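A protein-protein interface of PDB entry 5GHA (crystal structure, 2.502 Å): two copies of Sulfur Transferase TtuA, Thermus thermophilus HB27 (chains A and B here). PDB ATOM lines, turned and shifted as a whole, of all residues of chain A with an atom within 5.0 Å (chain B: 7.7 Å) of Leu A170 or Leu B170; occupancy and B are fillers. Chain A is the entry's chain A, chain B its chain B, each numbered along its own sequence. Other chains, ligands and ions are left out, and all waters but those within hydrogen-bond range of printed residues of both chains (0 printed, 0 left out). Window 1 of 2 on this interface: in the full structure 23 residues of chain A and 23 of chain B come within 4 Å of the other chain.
The backbone carbonyl oxygen (O) of Leu A171 sits at hydrogen-bond distance from the guanidinium group (NE) of Arg B250, 3.3 Å away. The side-chain amide nitrogen of Asn A172 sits close to the guanidinium group of Arg B250 (3.2 Å). The guanidinium group of Arg A250 lies within hydrogen-bond range of the side-chain amide oxygen of Asn B172 (3.2 Å).
The side-chain amide nitrogen of Asn B172 sits at hydrogen-bond distance from the backbone carbonyl oxygen of Gly B168 (2.9 Å). The backbone carbonyl oxygen (O) of Gly B254 lies within hydrogen-bond range of the backbone NH (N) of Ile B259 (3.2 Å).
Among the printed residues, pairs that only touch across the chains: Arg A250 with Leu B171, Pro A173 with Arg B250, Phe A251 with Leu B170, Leu A170 with Ile B259, Leu A170 with Phe B251, Arg A250 with Pro B173, Pro A173 with Gly B254, Phe A167 with Phe B167, Ile A259 with Leu B170, Phe A251 with Leu B171, Leu A170 with Leu B170 and Leu A171 with Ala B247.
Of the printed residues of chain B, Leu A170 touches Leu B170 (3.8 Å), Phe B251 (3.6 Å) and Ile B259 (3.6 Å). Leu B170 touches just these residues of chain A: Leu A170, Phe A251 and Ile A259. Of the printed residues of chain B, Leu A171 touches Ala B247 and Arg B250. Of the printed residues of chain A, Asn B172 touches Arg A250. Printed residues of chain B within 4 Å of Phe A251: Leu B170 (3.5 Å) and Leu B171 (3.8 Å). Printed residues of chain A within 4 Å of Ala B247: Leu A171 (3.96 Å). Val B165 touches none of the printed residues of chain A. Lys B248 touches none of the printed residues of chain A. The nearest printed residue of chain B that does not touch Leu A170 is Arg B250 (4.02 Å). The nearest residue of chain A that does not touch Leu B170 is Arg A250 (4.2 Å). The nearest printed residue of chain A that does not touch Asn B172 is Phe A251 (5.8 Å).
Printed residues of chain A that touch a printed residue of chain B: Phe A167, Leu A170, Leu A171, Asn A172, Pro A173, Arg A250, Phe A251 and Ile A259. Hydrophobic or aromatic side chains of chain A that line the printed part of chain B: Phe A167, Leu A170, Leu A171, Pro A173, Phe A251 and Ile A259. Along chain A the printed residues that touch a printed residue of chain B span positions 167 to 259. Among the printed residues, 15 pairs touch across the chains.
Phe A167 touches its own counterpart, Phe B167. Leu A170 touches its own counterpart, Leu B170. Asn A172 touches Arg B250, and with the chains exchanged Arg A250 touches Asn B172. Phe A251 touches Leu B171, but with the chains exchanged Leu A171 does not touch Phe B251 (4.1 Å). Positions printed for both chains: 166, 167, 168, 169, 170, 171, 172, 173, 250, 251 and 259. Of the 15 pairs that touch across the chains among the printed residues, 12 have their exchanged pair printed and touching as well.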
ATOM      1  N   LEU A 166      13.561 -17.909  13.244  1.00  0.00           N
ATOM      2  CA  LEU A 166      12.878 -17.992  14.534  1.00  0.00           C
ATOM      3  C   LEU A 166      11.520 -18.670  14.387  1.00  0.00           C
ATOM      4  O   LEU A 166      11.167 -19.546  15.174  1.00  0.00           O
ATOM      5  CB  LEU A 166      12.701 -16.603  15.151  1.00  0.00           C
ATOM      6  CG  LEU A 166      11.749 -16.539  16.349  1.00  0.00           C
ATOM      7  CD1 LEU A 166      12.248 -17.403  17.503  1.00  0.00           C
ATOM      8  CD2 LEU A 166      11.533 -15.101  16.799  1.00  0.00           C
ATOM      9  N   PHE A 167      10.771 -18.257  13.371  1.00  0.00           N
ATOM     10  CA  PHE A 167       9.473 -18.849  13.072  1.00  0.00           C
ATOM     11  C   PHE A 167       9.632 -20.324  12.728  1.00  0.00           C
ATOM     12  O   PHE A 167       8.820 -21.156  13.131  1.00  0.00           O
ATOM     13  CB  PHE A 167       8.799 -18.105  11.916  1.00  0.00           C
ATOM     14  CG  PHE A 167       7.334 -18.400  11.774  1.00  0.00           C
ATOM     15  CD1 PHE A 167       6.571 -18.743  12.877  1.00  0.00           C
ATOM     16  CD2 PHE A 167       6.719 -18.335  10.536  1.00  0.00           C
ATOM     17  CE1 PHE A 167       5.220 -19.012  12.747  1.00  0.00           C
ATOM     18  CE2 PHE A 167       5.368 -18.605  10.400  1.00  0.00           C
ATOM     19  CZ  PHE A 167       4.620 -18.945  11.506  1.00  0.00           C
ATOM     20  N   GLY A 168      10.685 -20.638  11.980  1.00  0.00           N
ATOM     21  CA  GLY A 168      10.983 -22.007  11.601  1.00  0.00           C
ATOM     22  C   GLY A 168      11.304 -22.872  12.804  1.00  0.00           C
ATOM     23  O   GLY A 168      10.967 -24.054  12.836  1.00  0.00           O
ATOM     24  N   ASN A 169      11.965 -22.280  13.794  1.00  0.00           N
ATOM     25  CA  ASN A 169      12.251 -22.968  15.047  1.00  0.00           C
ATOM     26  C   ASN A 169      10.970 -23.380  15.761  1.00  0.00           C
ATOM     27  O   ASN A 169      10.813 -24.532  16.161  1.00  0.00           O
ATOM     28  CB  ASN A 169      13.089 -22.083  15.974  1.00  0.00           C
ATOM     29  CG  ASN A 169      14.568 -22.141  15.658  1.00  0.00           C
ATOM     30  OD1 ASN A 169      14.972 -22.615  14.595  1.00  0.00           O
ATOM     31  ND2 ASN A 169      15.388 -21.659  16.585  1.00  0.00           N
ATOM     32  N   LEU A 170      10.062 -22.423  15.916  1.00  0.00           N
ATOM     33  CA  LEU A 170       8.794 -22.653  16.602  1.00  0.00           C
ATOM     34  C   LEU A 170       7.929 -23.665  15.857  1.00  0.00           C
ATOM     35  O   LEU A 170       7.288 -24.515  16.471  1.00  0.00           O
ATOM     36  CB  LEU A 170       8.042 -21.333  16.768  1.00  0.00           C
ATOM     37  CG  LEU A 170       8.865 -20.223  17.426  1.00  0.00           C
ATOM     38  CD1 LEU A 170       8.158 -18.880  17.333  1.00  0.00           C
ATOM     39  CD2 LEU A 170       9.159 -20.573  18.873  1.00  0.00           C
ATOM     40  N   LEU A 171       7.926 -23.575  14.532  1.00  0.00           N
ATOM     41  CA  LEU A 171       7.147 -24.489  13.703  1.00  0.00           C
ATOM     42  C   LEU A 171       7.704 -25.914  13.727  1.00  0.00           C
ATOM     43  O   LEU A 171       6.962 -26.877  13.528  1.00  0.00           O
ATOM     44  CB  LEU A 171       7.084 -23.977  12.262  1.00  0.00           C
ATOM     45  CG  LEU A 171       6.109 -22.824  12.013  1.00  0.00           C
ATOM     46  CD1 LEU A 171       6.174 -22.355  10.570  1.00  0.00           C
ATOM     47  CD2 LEU A 171       4.694 -23.245  12.372  1.00  0.00           C
ATOM     48  N   ASN A 172       9.004 -26.046  13.968  1.00  0.00           N
ATOM     49  CA  ASN A 172       9.636 -27.359  14.042  1.00  0.00           C
ATOM     50  C   ASN A 172      10.525 -27.507  15.272  1.00  0.00           C
ATOM     51  O   ASN A 172      11.749 -27.482  15.158  1.00  0.00           O
ATOM     52  CB  ASN A 172      10.461 -27.631  12.782  1.00  0.00           C
ATOM     53  CG  ASN A 172       9.621 -27.631  11.521  1.00  0.00           C
ATOM     54  OD1 ASN A 172       9.485 -26.606  10.853  1.00  0.00           O
ATOM     55  ND2 ASN A 172       9.056 -28.787  11.184  1.00  0.00           N
ATOM     56  N   PRO A 173       9.913 -27.660  16.455  1.00  0.00           N
ATOM     57  CA  PRO A 173      10.687 -27.829  17.689  1.00  0.00           C
ATOM     58  C   PRO A 173      11.386 -29.184  17.748  1.00  0.00           C
ATOM     59  O   PRO A 173      12.221 -29.389  18.629  1.00  0.00           O
ATOM     60  CB  PRO A 173       9.626 -27.710  18.786  1.00  0.00           C
ATOM     61  CG  PRO A 173       8.366 -28.163  18.129  1.00  0.00           C
ATOM     62  CD  PRO A 173       8.460 -27.682  16.709  1.00  0.00           C
ATOM     63  N   ARG A 250       8.602  -6.623  15.817  1.00  0.00           N
ATOM     64  CA  ARG A 250       8.041  -6.915  17.132  1.00  0.00           C
ATOM     65  C   ARG A 250       8.204  -8.393  17.456  1.00  0.00           C
ATOM     66  O   ARG A 250       8.485  -8.765  18.595  1.00  0.00           O
ATOM     67  CB  ARG A 250       6.566  -6.513  17.202  1.00  0.00           C
ATOM     68  CG  ARG A 250       6.316  -5.027  17.008  1.00  0.00           C
ATOM     69  CD  ARG A 250       4.932  -4.621  17.493  1.00  0.00           C
ATOM     70  NE  ARG A 250       3.859  -5.284  16.756  1.00  0.00           N
ATOM     71  CZ  ARG A 250       3.368  -4.850  15.599  1.00  0.00           C
ATOM     72  NH1 ARG A 250       3.859  -3.755  15.031  1.00  0.00           N
ATOM     73  NH2 ARG A 250       2.389  -5.517  15.003  1.00  0.00           N
ATOM     74  N   PHE A 251       8.032  -9.226  16.436  1.00  0.00           N
ATOM     75  CA  PHE A 251       8.211 -10.667  16.567  1.00  0.00           C
ATOM     76  C   PHE A 251       9.628 -11.010  17.018  1.00  0.00           C
ATOM     77  O   PHE A 251       9.826 -11.602  18.081  1.00  0.00           O
ATOM     78  CB  PHE A 251       7.893 -11.349  15.235  1.00  0.00           C
ATOM     79  CG  PHE A 251       8.009 -12.846  15.265  1.00  0.00           C
ATOM     80  CD1 PHE A 251       7.245 -13.599  16.141  1.00  0.00           C
ATOM     81  CD2 PHE A 251       8.860 -13.502  14.392  1.00  0.00           C
ATOM     82  CE1 PHE A 251       7.345 -14.976  16.159  1.00  0.00           C
ATOM     83  CE2 PHE A 251       8.962 -14.881  14.402  1.00  0.00           C
ATOM     84  CZ  PHE A 251       8.204 -15.619  15.287  1.00  0.00           C
ATOM     85  N   ILE A 259      11.570 -12.775  25.759  1.00  0.00           N
ATOM     86  CA  ILE A 259      11.324 -14.201  25.969  1.00  0.00           C
ATOM     87  C   ILE A 259      12.591 -14.984  26.304  1.00  0.00           C
ATOM     88  O   ILE A 259      12.667 -15.623  27.351  1.00  0.00           O
ATOM     89  CB  ILE A 259      10.654 -14.840  24.737  1.00  0.00           C
ATOM     90  CG1 ILE A 259       9.231 -14.302  24.574  1.00  0.00           C
ATOM     91  CG2 ILE A 259      10.630 -16.358  24.863  1.00  0.00           C
ATOM     92  CD1 ILE A 259       8.500 -14.855  23.374  1.00  0.00           C
ATOM     93  N   ALA B 163      -3.578 -21.937  18.185  1.00  0.00           N
ATOM     94  CA  ALA B 163      -2.317 -21.601  17.534  1.00  0.00           C
ATOM     95  C   ALA B 163      -2.280 -20.131  17.123  1.00  0.00           C
ATOM     96  O   ALA B 163      -1.215 -19.514  17.092  1.00  0.00           O
ATOM     97  CB  ALA B 163      -2.086 -22.497  16.323  1.00  0.00           C
ATOM     98  N   ALA B 164      -3.448 -19.575  16.809  1.00  0.00           N
ATOM     99  CA  ALA B 164      -3.544 -18.177  16.401  1.00  0.00           C
ATOM    100  C   ALA B 164      -3.361 -17.245  17.591  1.00  0.00           C
ATOM    101  O   ALA B 164      -2.764 -16.178  17.467  1.00  0.00           O
ATOM    102  CB  ALA B 164      -4.872 -17.911  15.721  1.00  0.00           C
ATOM    103  N   VAL B 165      -3.885 -17.653  18.743  1.00  0.00           N
ATOM    104  CA  VAL B 165      -3.741 -16.873  19.967  1.00  0.00           C
ATOM    105  C   VAL B 165      -2.282 -16.866  20.410  1.00  0.00           C
ATOM    106  O   VAL B 165      -1.747 -15.831  20.807  1.00  0.00           O
ATOM    107  CB  VAL B 165      -4.632 -17.424  21.101  1.00  0.00           C
ATOM    108  CG1 VAL B 165      -4.276 -16.782  22.431  1.00  0.00           C
ATOM    109  CG2 VAL B 165      -6.091 -17.192  20.778  1.00  0.00           C
ATOM    110  N   LEU B 166      -1.643 -18.027  20.327  1.00  0.00           N
ATOM    111  CA  LEU B 166      -0.227 -18.154  20.645  1.00  0.00           C
ATOM    112  C   LEU B 166       0.622 -17.319  19.691  1.00  0.00           C
ATOM    113  O   LEU B 166       1.535 -16.611  20.114  1.00  0.00           O
ATOM    114  CB  LEU B 166       0.204 -19.621  20.588  1.00  0.00           C
ATOM    115  CG  LEU B 166       1.701 -19.887  20.749  1.00  0.00           C
ATOM    116  CD1 LEU B 166       2.198 -19.415  22.111  1.00  0.00           C
ATOM    117  CD2 LEU B 166       2.009 -21.365  20.536  1.00  0.00           C
ATOM    118  N   PHE B 167       0.306 -17.403  18.402  1.00  0.00           N
ATOM    119  CA  PHE B 167       1.020 -16.651  17.380  1.00  0.00           C
ATOM    120  C   PHE B 167       0.906 -15.147  17.615  1.00  0.00           C
ATOM    121  O   PHE B 167       1.902 -14.422  17.558  1.00  0.00           O
ATOM    122  CB  PHE B 167       0.488 -17.002  15.990  1.00  0.00           C
ATOM    123  CG  PHE B 167       1.382 -16.556  14.867  1.00  0.00           C
ATOM    124  CD1 PHE B 167       2.738 -16.361  15.077  1.00  0.00           C
ATOM    125  CD2 PHE B 167       0.863 -16.325  13.605  1.00  0.00           C
ATOM    126  CE1 PHE B 167       3.560 -15.949  14.045  1.00  0.00           C
ATOM    127  CE2 PHE B 167       1.682 -15.913  12.571  1.00  0.00           C
ATOM    128  CZ  PHE B 167       3.032 -15.725  12.793  1.00  0.00           C
ATOM    129  N   GLY B 168      -0.317 -14.691  17.875  1.00  0.00           N
ATOM    130  CA  GLY B 168      -0.582 -13.287  18.113  1.00  0.00           C
ATOM    131  C   GLY B 168       0.166 -12.752  19.314  1.00  0.00           C
ATOM    132  O   GLY B 168       0.596 -11.599  19.322  1.00  0.00           O
ATOM    133  N   ASN B 169       0.318 -13.589  20.335  1.00  0.00           N
ATOM    134  CA  ASN B 169       1.115 -13.226  21.501  1.00  0.00           C
ATOM    135  C   ASN B 169       2.568 -12.980  21.119  1.00  0.00           C
ATOM    136  O   ASN B 169       3.159 -11.978  21.517  1.00  0.00           O
ATOM    137  CB  ASN B 169       1.033 -14.314  22.574  1.00  0.00           C
ATOM    138  CG  ASN B 169      -0.306 -14.331  23.290  1.00  0.00           C
ATOM    139  OD1 ASN B 169      -1.050 -13.352  23.260  1.00  0.00           O
ATOM    140  ND2 ASN B 169      -0.615 -15.444  23.945  1.00  0.00           N
ATOM    141  N   LEU B 170       3.132 -13.899  20.340  1.00  0.00           N
ATOM    142  CA  LEU B 170       4.528 -13.807  19.920  1.00  0.00           C
ATOM    143  C   LEU B 170       4.746 -12.629  18.975  1.00  0.00           C
ATOM    144  O   LEU B 170       5.815 -12.021  18.966  1.00  0.00           O
ATOM    145  CB  LEU B 170       4.971 -15.110  19.249  1.00  0.00           C
ATOM    146  CG  LEU B 170       4.834 -16.373  20.101  1.00  0.00           C
ATOM    147  CD1 LEU B 170       5.121 -17.617  19.283  1.00  0.00           C
ATOM    148  CD2 LEU B 170       5.749 -16.304  21.310  1.00  0.00           C
ATOM    149  N   LEU B 171       3.726 -12.310  18.185  1.00  0.00           N
ATOM    150  CA  LEU B 171       3.807 -11.200  17.245  1.00  0.00           C
ATOM    151  C   LEU B 171       3.703  -9.863  17.966  1.00  0.00           C
ATOM    152  O   LEU B 171       4.416  -8.913  17.639  1.00  0.00           O
ATOM    153  CB  LEU B 171       2.711 -11.311  16.185  1.00  0.00           C
ATOM    154  CG  LEU B 171       2.956 -12.344  15.086  1.00  0.00           C
ATOM    155  CD1 LEU B 171       1.728 -12.501  14.205  1.00  0.00           C
ATOM    156  CD2 LEU B 171       4.164 -11.941  14.258  1.00  0.00           C
ATOM    157  N   ASN B 172       2.810  -9.797  18.950  1.00  0.00           N
ATOM    158  CA  ASN B 172       2.625  -8.588  19.744  1.00  0.00           C
ATOM    159  C   ASN B 172       2.896  -8.850  21.225  1.00  0.00           C
ATOM    160  O   ASN B 172       1.970  -8.860  22.036  1.00  0.00           O
ATOM    161  CB  ASN B 172       1.205  -8.042  19.564  1.00  0.00           C
ATOM    162  CG  ASN B 172       0.728  -8.114  18.123  1.00  0.00           C
ATOM    163  OD1 ASN B 172       0.980  -7.209  17.326  1.00  0.00           O
ATOM    164  ND2 ASN B 172       0.028  -9.190  17.784  1.00  0.00           N
ATOM    165  N   PRO B 173       4.172  -9.059  21.584  1.00  0.00           N
ATOM    166  CA  PRO B 173       4.519  -9.453  22.953  1.00  0.00           C
ATOM    167  C   PRO B 173       4.495  -8.284  23.930  1.00  0.00           C
ATOM    168  O   PRO B 173       5.025  -8.435  25.030  1.00  0.00           O
ATOM    169  CB  PRO B 173       5.934 -10.003  22.800  1.00  0.00           C
ATOM    170  CG  PRO B 173       6.511  -9.191  21.693  1.00  0.00           C
ATOM    171  CD  PRO B 173       5.372  -8.887  20.745  1.00  0.00           C
ATOM    172  N   ALA B 247       2.151 -28.623  10.896  1.00  0.00           N
ATOM    173  CA  ALA B 247       2.901 -27.505  11.463  1.00  0.00           C
ATOM    174  C   ALA B 247       2.197 -26.846  12.652  1.00  0.00           C
ATOM    175  O   ALA B 247       2.838 -26.505  13.644  1.00  0.00           O
ATOM    176  CB  ALA B 247       3.181 -26.467  10.385  1.00  0.00           C
ATOM    177  N   LYS B 248       0.884 -26.665  12.547  1.00  0.00           N
ATOM    178  CA  LYS B 248       0.119 -26.010  13.606  1.00  0.00           C
ATOM    179  C   LYS B 248       0.175 -26.796  14.913  1.00  0.00           C
ATOM    180  O   LYS B 248       0.276 -26.212  15.991  1.00  0.00           O
ATOM    181  CB  LYS B 248      -1.338 -25.811  13.177  1.00  0.00           C
ATOM    182  CG  LYS B 248      -1.535 -24.711  12.151  1.00  0.00           C
ATOM    183  CD  LYS B 248      -3.006 -24.524  11.790  1.00  0.00           C
ATOM    184  CE  LYS B 248      -3.571 -25.749  11.082  1.00  0.00           C
ATOM    185  NZ  LYS B 248      -4.890 -25.471  10.441  1.00  0.00           N
ATOM    186  N   LEU B 249       0.114 -28.119  14.815  1.00  0.00           N
ATOM    187  CA  LEU B 249       0.198 -28.968  15.999  1.00  0.00           C
ATOM    188  C   LEU B 249       1.610 -28.970  16.580  1.00  0.00           C
ATOM    189  O   LEU B 249       1.783 -28.934  17.798  1.00  0.00           O
ATOM    190  CB  LEU B 249      -0.240 -30.397  15.673  1.00  0.00           C
ATOM    191  CG  LEU B 249      -0.343 -31.335  16.875  1.00  0.00           C
ATOM    192  CD1 LEU B 249      -1.273 -30.746  17.919  1.00  0.00           C
ATOM    193  CD2 LEU B 249      -0.820 -32.716  16.446  1.00  0.00           C
ATOM    194  N   ARG B 250       2.616 -29.013  15.710  1.00  0.00           N
ATOM    195  CA  ARG B 250       4.007 -28.943  16.151  1.00  0.00           C
ATOM    196  C   ARG B 250       4.275 -27.616  16.847  1.00  0.00           C
ATOM    197  O   ARG B 250       5.030 -27.550  17.818  1.00  0.00           O
ATOM    198  CB  ARG B 250       4.968 -29.120  14.973  1.00  0.00           C
ATOM    199  CG  ARG B 250       5.009 -30.526  14.402  1.00  0.00           C
ATOM    200  CD  ARG B 250       6.273 -30.767  13.585  1.00  0.00           C
ATOM    201  NE  ARG B 250       6.346 -29.924  12.396  1.00  0.00           N
ATOM    202  CZ  ARG B 250       5.801 -30.238  11.224  1.00  0.00           C
ATOM    203  NH1 ARG B 250       5.136 -31.377  11.083  1.00  0.00           N
ATOM    204  NH2 ARG B 250       5.918 -29.411  10.192  1.00  0.00           N
ATOM    205  N   PHE B 251       3.642 -26.566  16.340  1.00  0.00           N
ATOM    206  CA  PHE B 251       3.777 -25.224  16.890  1.00  0.00           C
ATOM    207  C   PHE B 251       3.202 -25.147  18.304  1.00  0.00           C
ATOM    208  O   PHE B 251       3.876 -24.701  19.232  1.00  0.00           O
ATOM    209  CB  PHE B 251       3.087 -24.220  15.964  1.00  0.00           C
ATOM    210  CG  PHE B 251       3.144 -22.798  16.444  1.00  0.00           C
ATOM    211  CD1 PHE B 251       4.357 -22.194  16.729  1.00  0.00           C
ATOM    212  CD2 PHE B 251       1.979 -22.054  16.577  1.00  0.00           C
ATOM    213  CE1 PHE B 251       4.408 -20.878  17.158  1.00  0.00           C
ATOM    214  CE2 PHE B 251       2.024 -20.736  17.004  1.00  0.00           C
ATOM    215  CZ  PHE B 251       3.238 -20.149  17.295  1.00  0.00           C
ATOM    216  N   LEU B 252       1.963 -25.602  18.462  1.00  0.00           N
ATOM    217  CA  LEU B 252       1.282 -25.551  19.752  1.00  0.00           C
ATOM    218  C   LEU B 252       1.897 -26.518  20.766  1.00  0.00           C
ATOM    219  O   LEU B 252       2.081 -26.166  21.931  1.00  0.00           O
ATOM    220  CB  LEU B 252      -0.209 -25.851  19.576  1.00  0.00           C
ATOM    221  CG  LEU B 252      -1.079 -25.742  20.831  1.00  0.00           C
ATOM    222  CD1 LEU B 252      -0.947 -24.361  21.462  1.00  0.00           C
ATOM    223  CD2 LEU B 252      -2.531 -26.047  20.503  1.00  0.00           C
ATOM    224  N   ASP B 253       2.209 -27.734  20.325  1.00  0.00           N
ATOM    225  CA  ASP B 253       2.844 -28.718  21.198  1.00  0.00           C
ATOM    226  C   ASP B 253       4.235 -28.273  21.623  1.00  0.00           C
ATOM    227  O   ASP B 253       4.651 -28.513  22.754  1.00  0.00           O
ATOM    228  CB  ASP B 253       2.927 -30.081  20.512  1.00  0.00           C
ATOM    229  CG  ASP B 253       1.720 -30.948  20.797  1.00  0.00           C
ATOM    230  OD1 ASP B 253       0.714 -30.415  21.313  1.00  0.00           O
ATOM    231  OD2 ASP B 253       1.777 -32.162  20.506  1.00  0.00           O
ATOM    232  N   GLY B 254       4.949 -27.621  20.709  1.00  0.00           N
ATOM    233  CA  GLY B 254       6.277 -27.118  20.997  1.00  0.00           C
ATOM    234  C   GLY B 254       6.283 -26.099  22.119  1.00  0.00           C
ATOM    235  O   GLY B 254       7.199 -26.069  22.939  1.00  0.00           O
ATOM    236  N   PHE B 255       5.255 -25.260  22.159  1.00  0.00           N
ATOM    237  CA  PHE B 255       5.157 -24.239  23.195  1.00  0.00           C
ATOM    238  C   PHE B 255       4.820 -24.854  24.549  1.00  0.00           C
ATOM    239  O   PHE B 255       5.342 -24.433  25.579  1.00  0.00           O
ATOM    240  CB  PHE B 255       4.109 -23.195  22.818  1.00  0.00           C
ATOM    241  CG  PHE B 255       3.912 -22.133  23.859  1.00  0.00           C
ATOM    242  CD1 PHE B 255       4.798 -21.076  23.964  1.00  0.00           C
ATOM    243  CD2 PHE B 255       2.832 -22.186  24.728  1.00  0.00           C
ATOM    244  CE1 PHE B 255       4.616 -20.093  24.921  1.00  0.00           C
ATOM    245  CE2 PHE B 255       2.645 -21.207  25.687  1.00  0.00           C
ATOM    246  CZ  PHE B 255       3.540 -20.159  25.783  1.00  0.00           C
ATOM    247  N   ILE B 259       8.853 -24.813  25.392  1.00  0.00           N
ATOM    248  CA  ILE B 259       9.061 -23.404  25.722  1.00  0.00           C
ATOM    249  C   ILE B 259       8.509 -23.006  27.091  1.00  0.00           C
ATOM    250  O   ILE B 259       9.257 -22.531  27.946  1.00  0.00           O
ATOM    251  CB  ILE B 259       8.439 -22.478  24.662  1.00  0.00           C
ATOM    252  CG1 ILE B 259       9.067 -22.741  23.293  1.00  0.00           C
ATOM    253  CG2 ILE B 259       8.625 -21.017  25.057  1.00  0.00           C
ATOM    254  CD1 ILE B 259       8.615 -21.778  22.222  1.00  0.00           C
ATOM    255  N   LEU B 263      10.025 -21.504  30.823  1.00  0.00           N
ATOM    256  CA  LEU B 263       9.752 -20.072  30.827  1.00  0.00           C
ATOM    257  C   LEU B 263       9.474 -19.512  32.221  1.00  0.00           C
ATOM    258  O   LEU B 263       8.492 -19.876  32.867  1.00  0.00           O
ATOM    259  CB  LEU B 263       8.571 -19.776  29.902  1.00  0.00           C
ATOM    260  CG  LEU B 263       8.327 -18.323  29.501  1.00  0.00           C
ATOM    261  CD1 LEU B 263       9.609 -17.696  28.979  1.00  0.00           C
ATOM    262  CD2 LEU B 263       7.233 -18.260  28.448  1.00  0.00           C
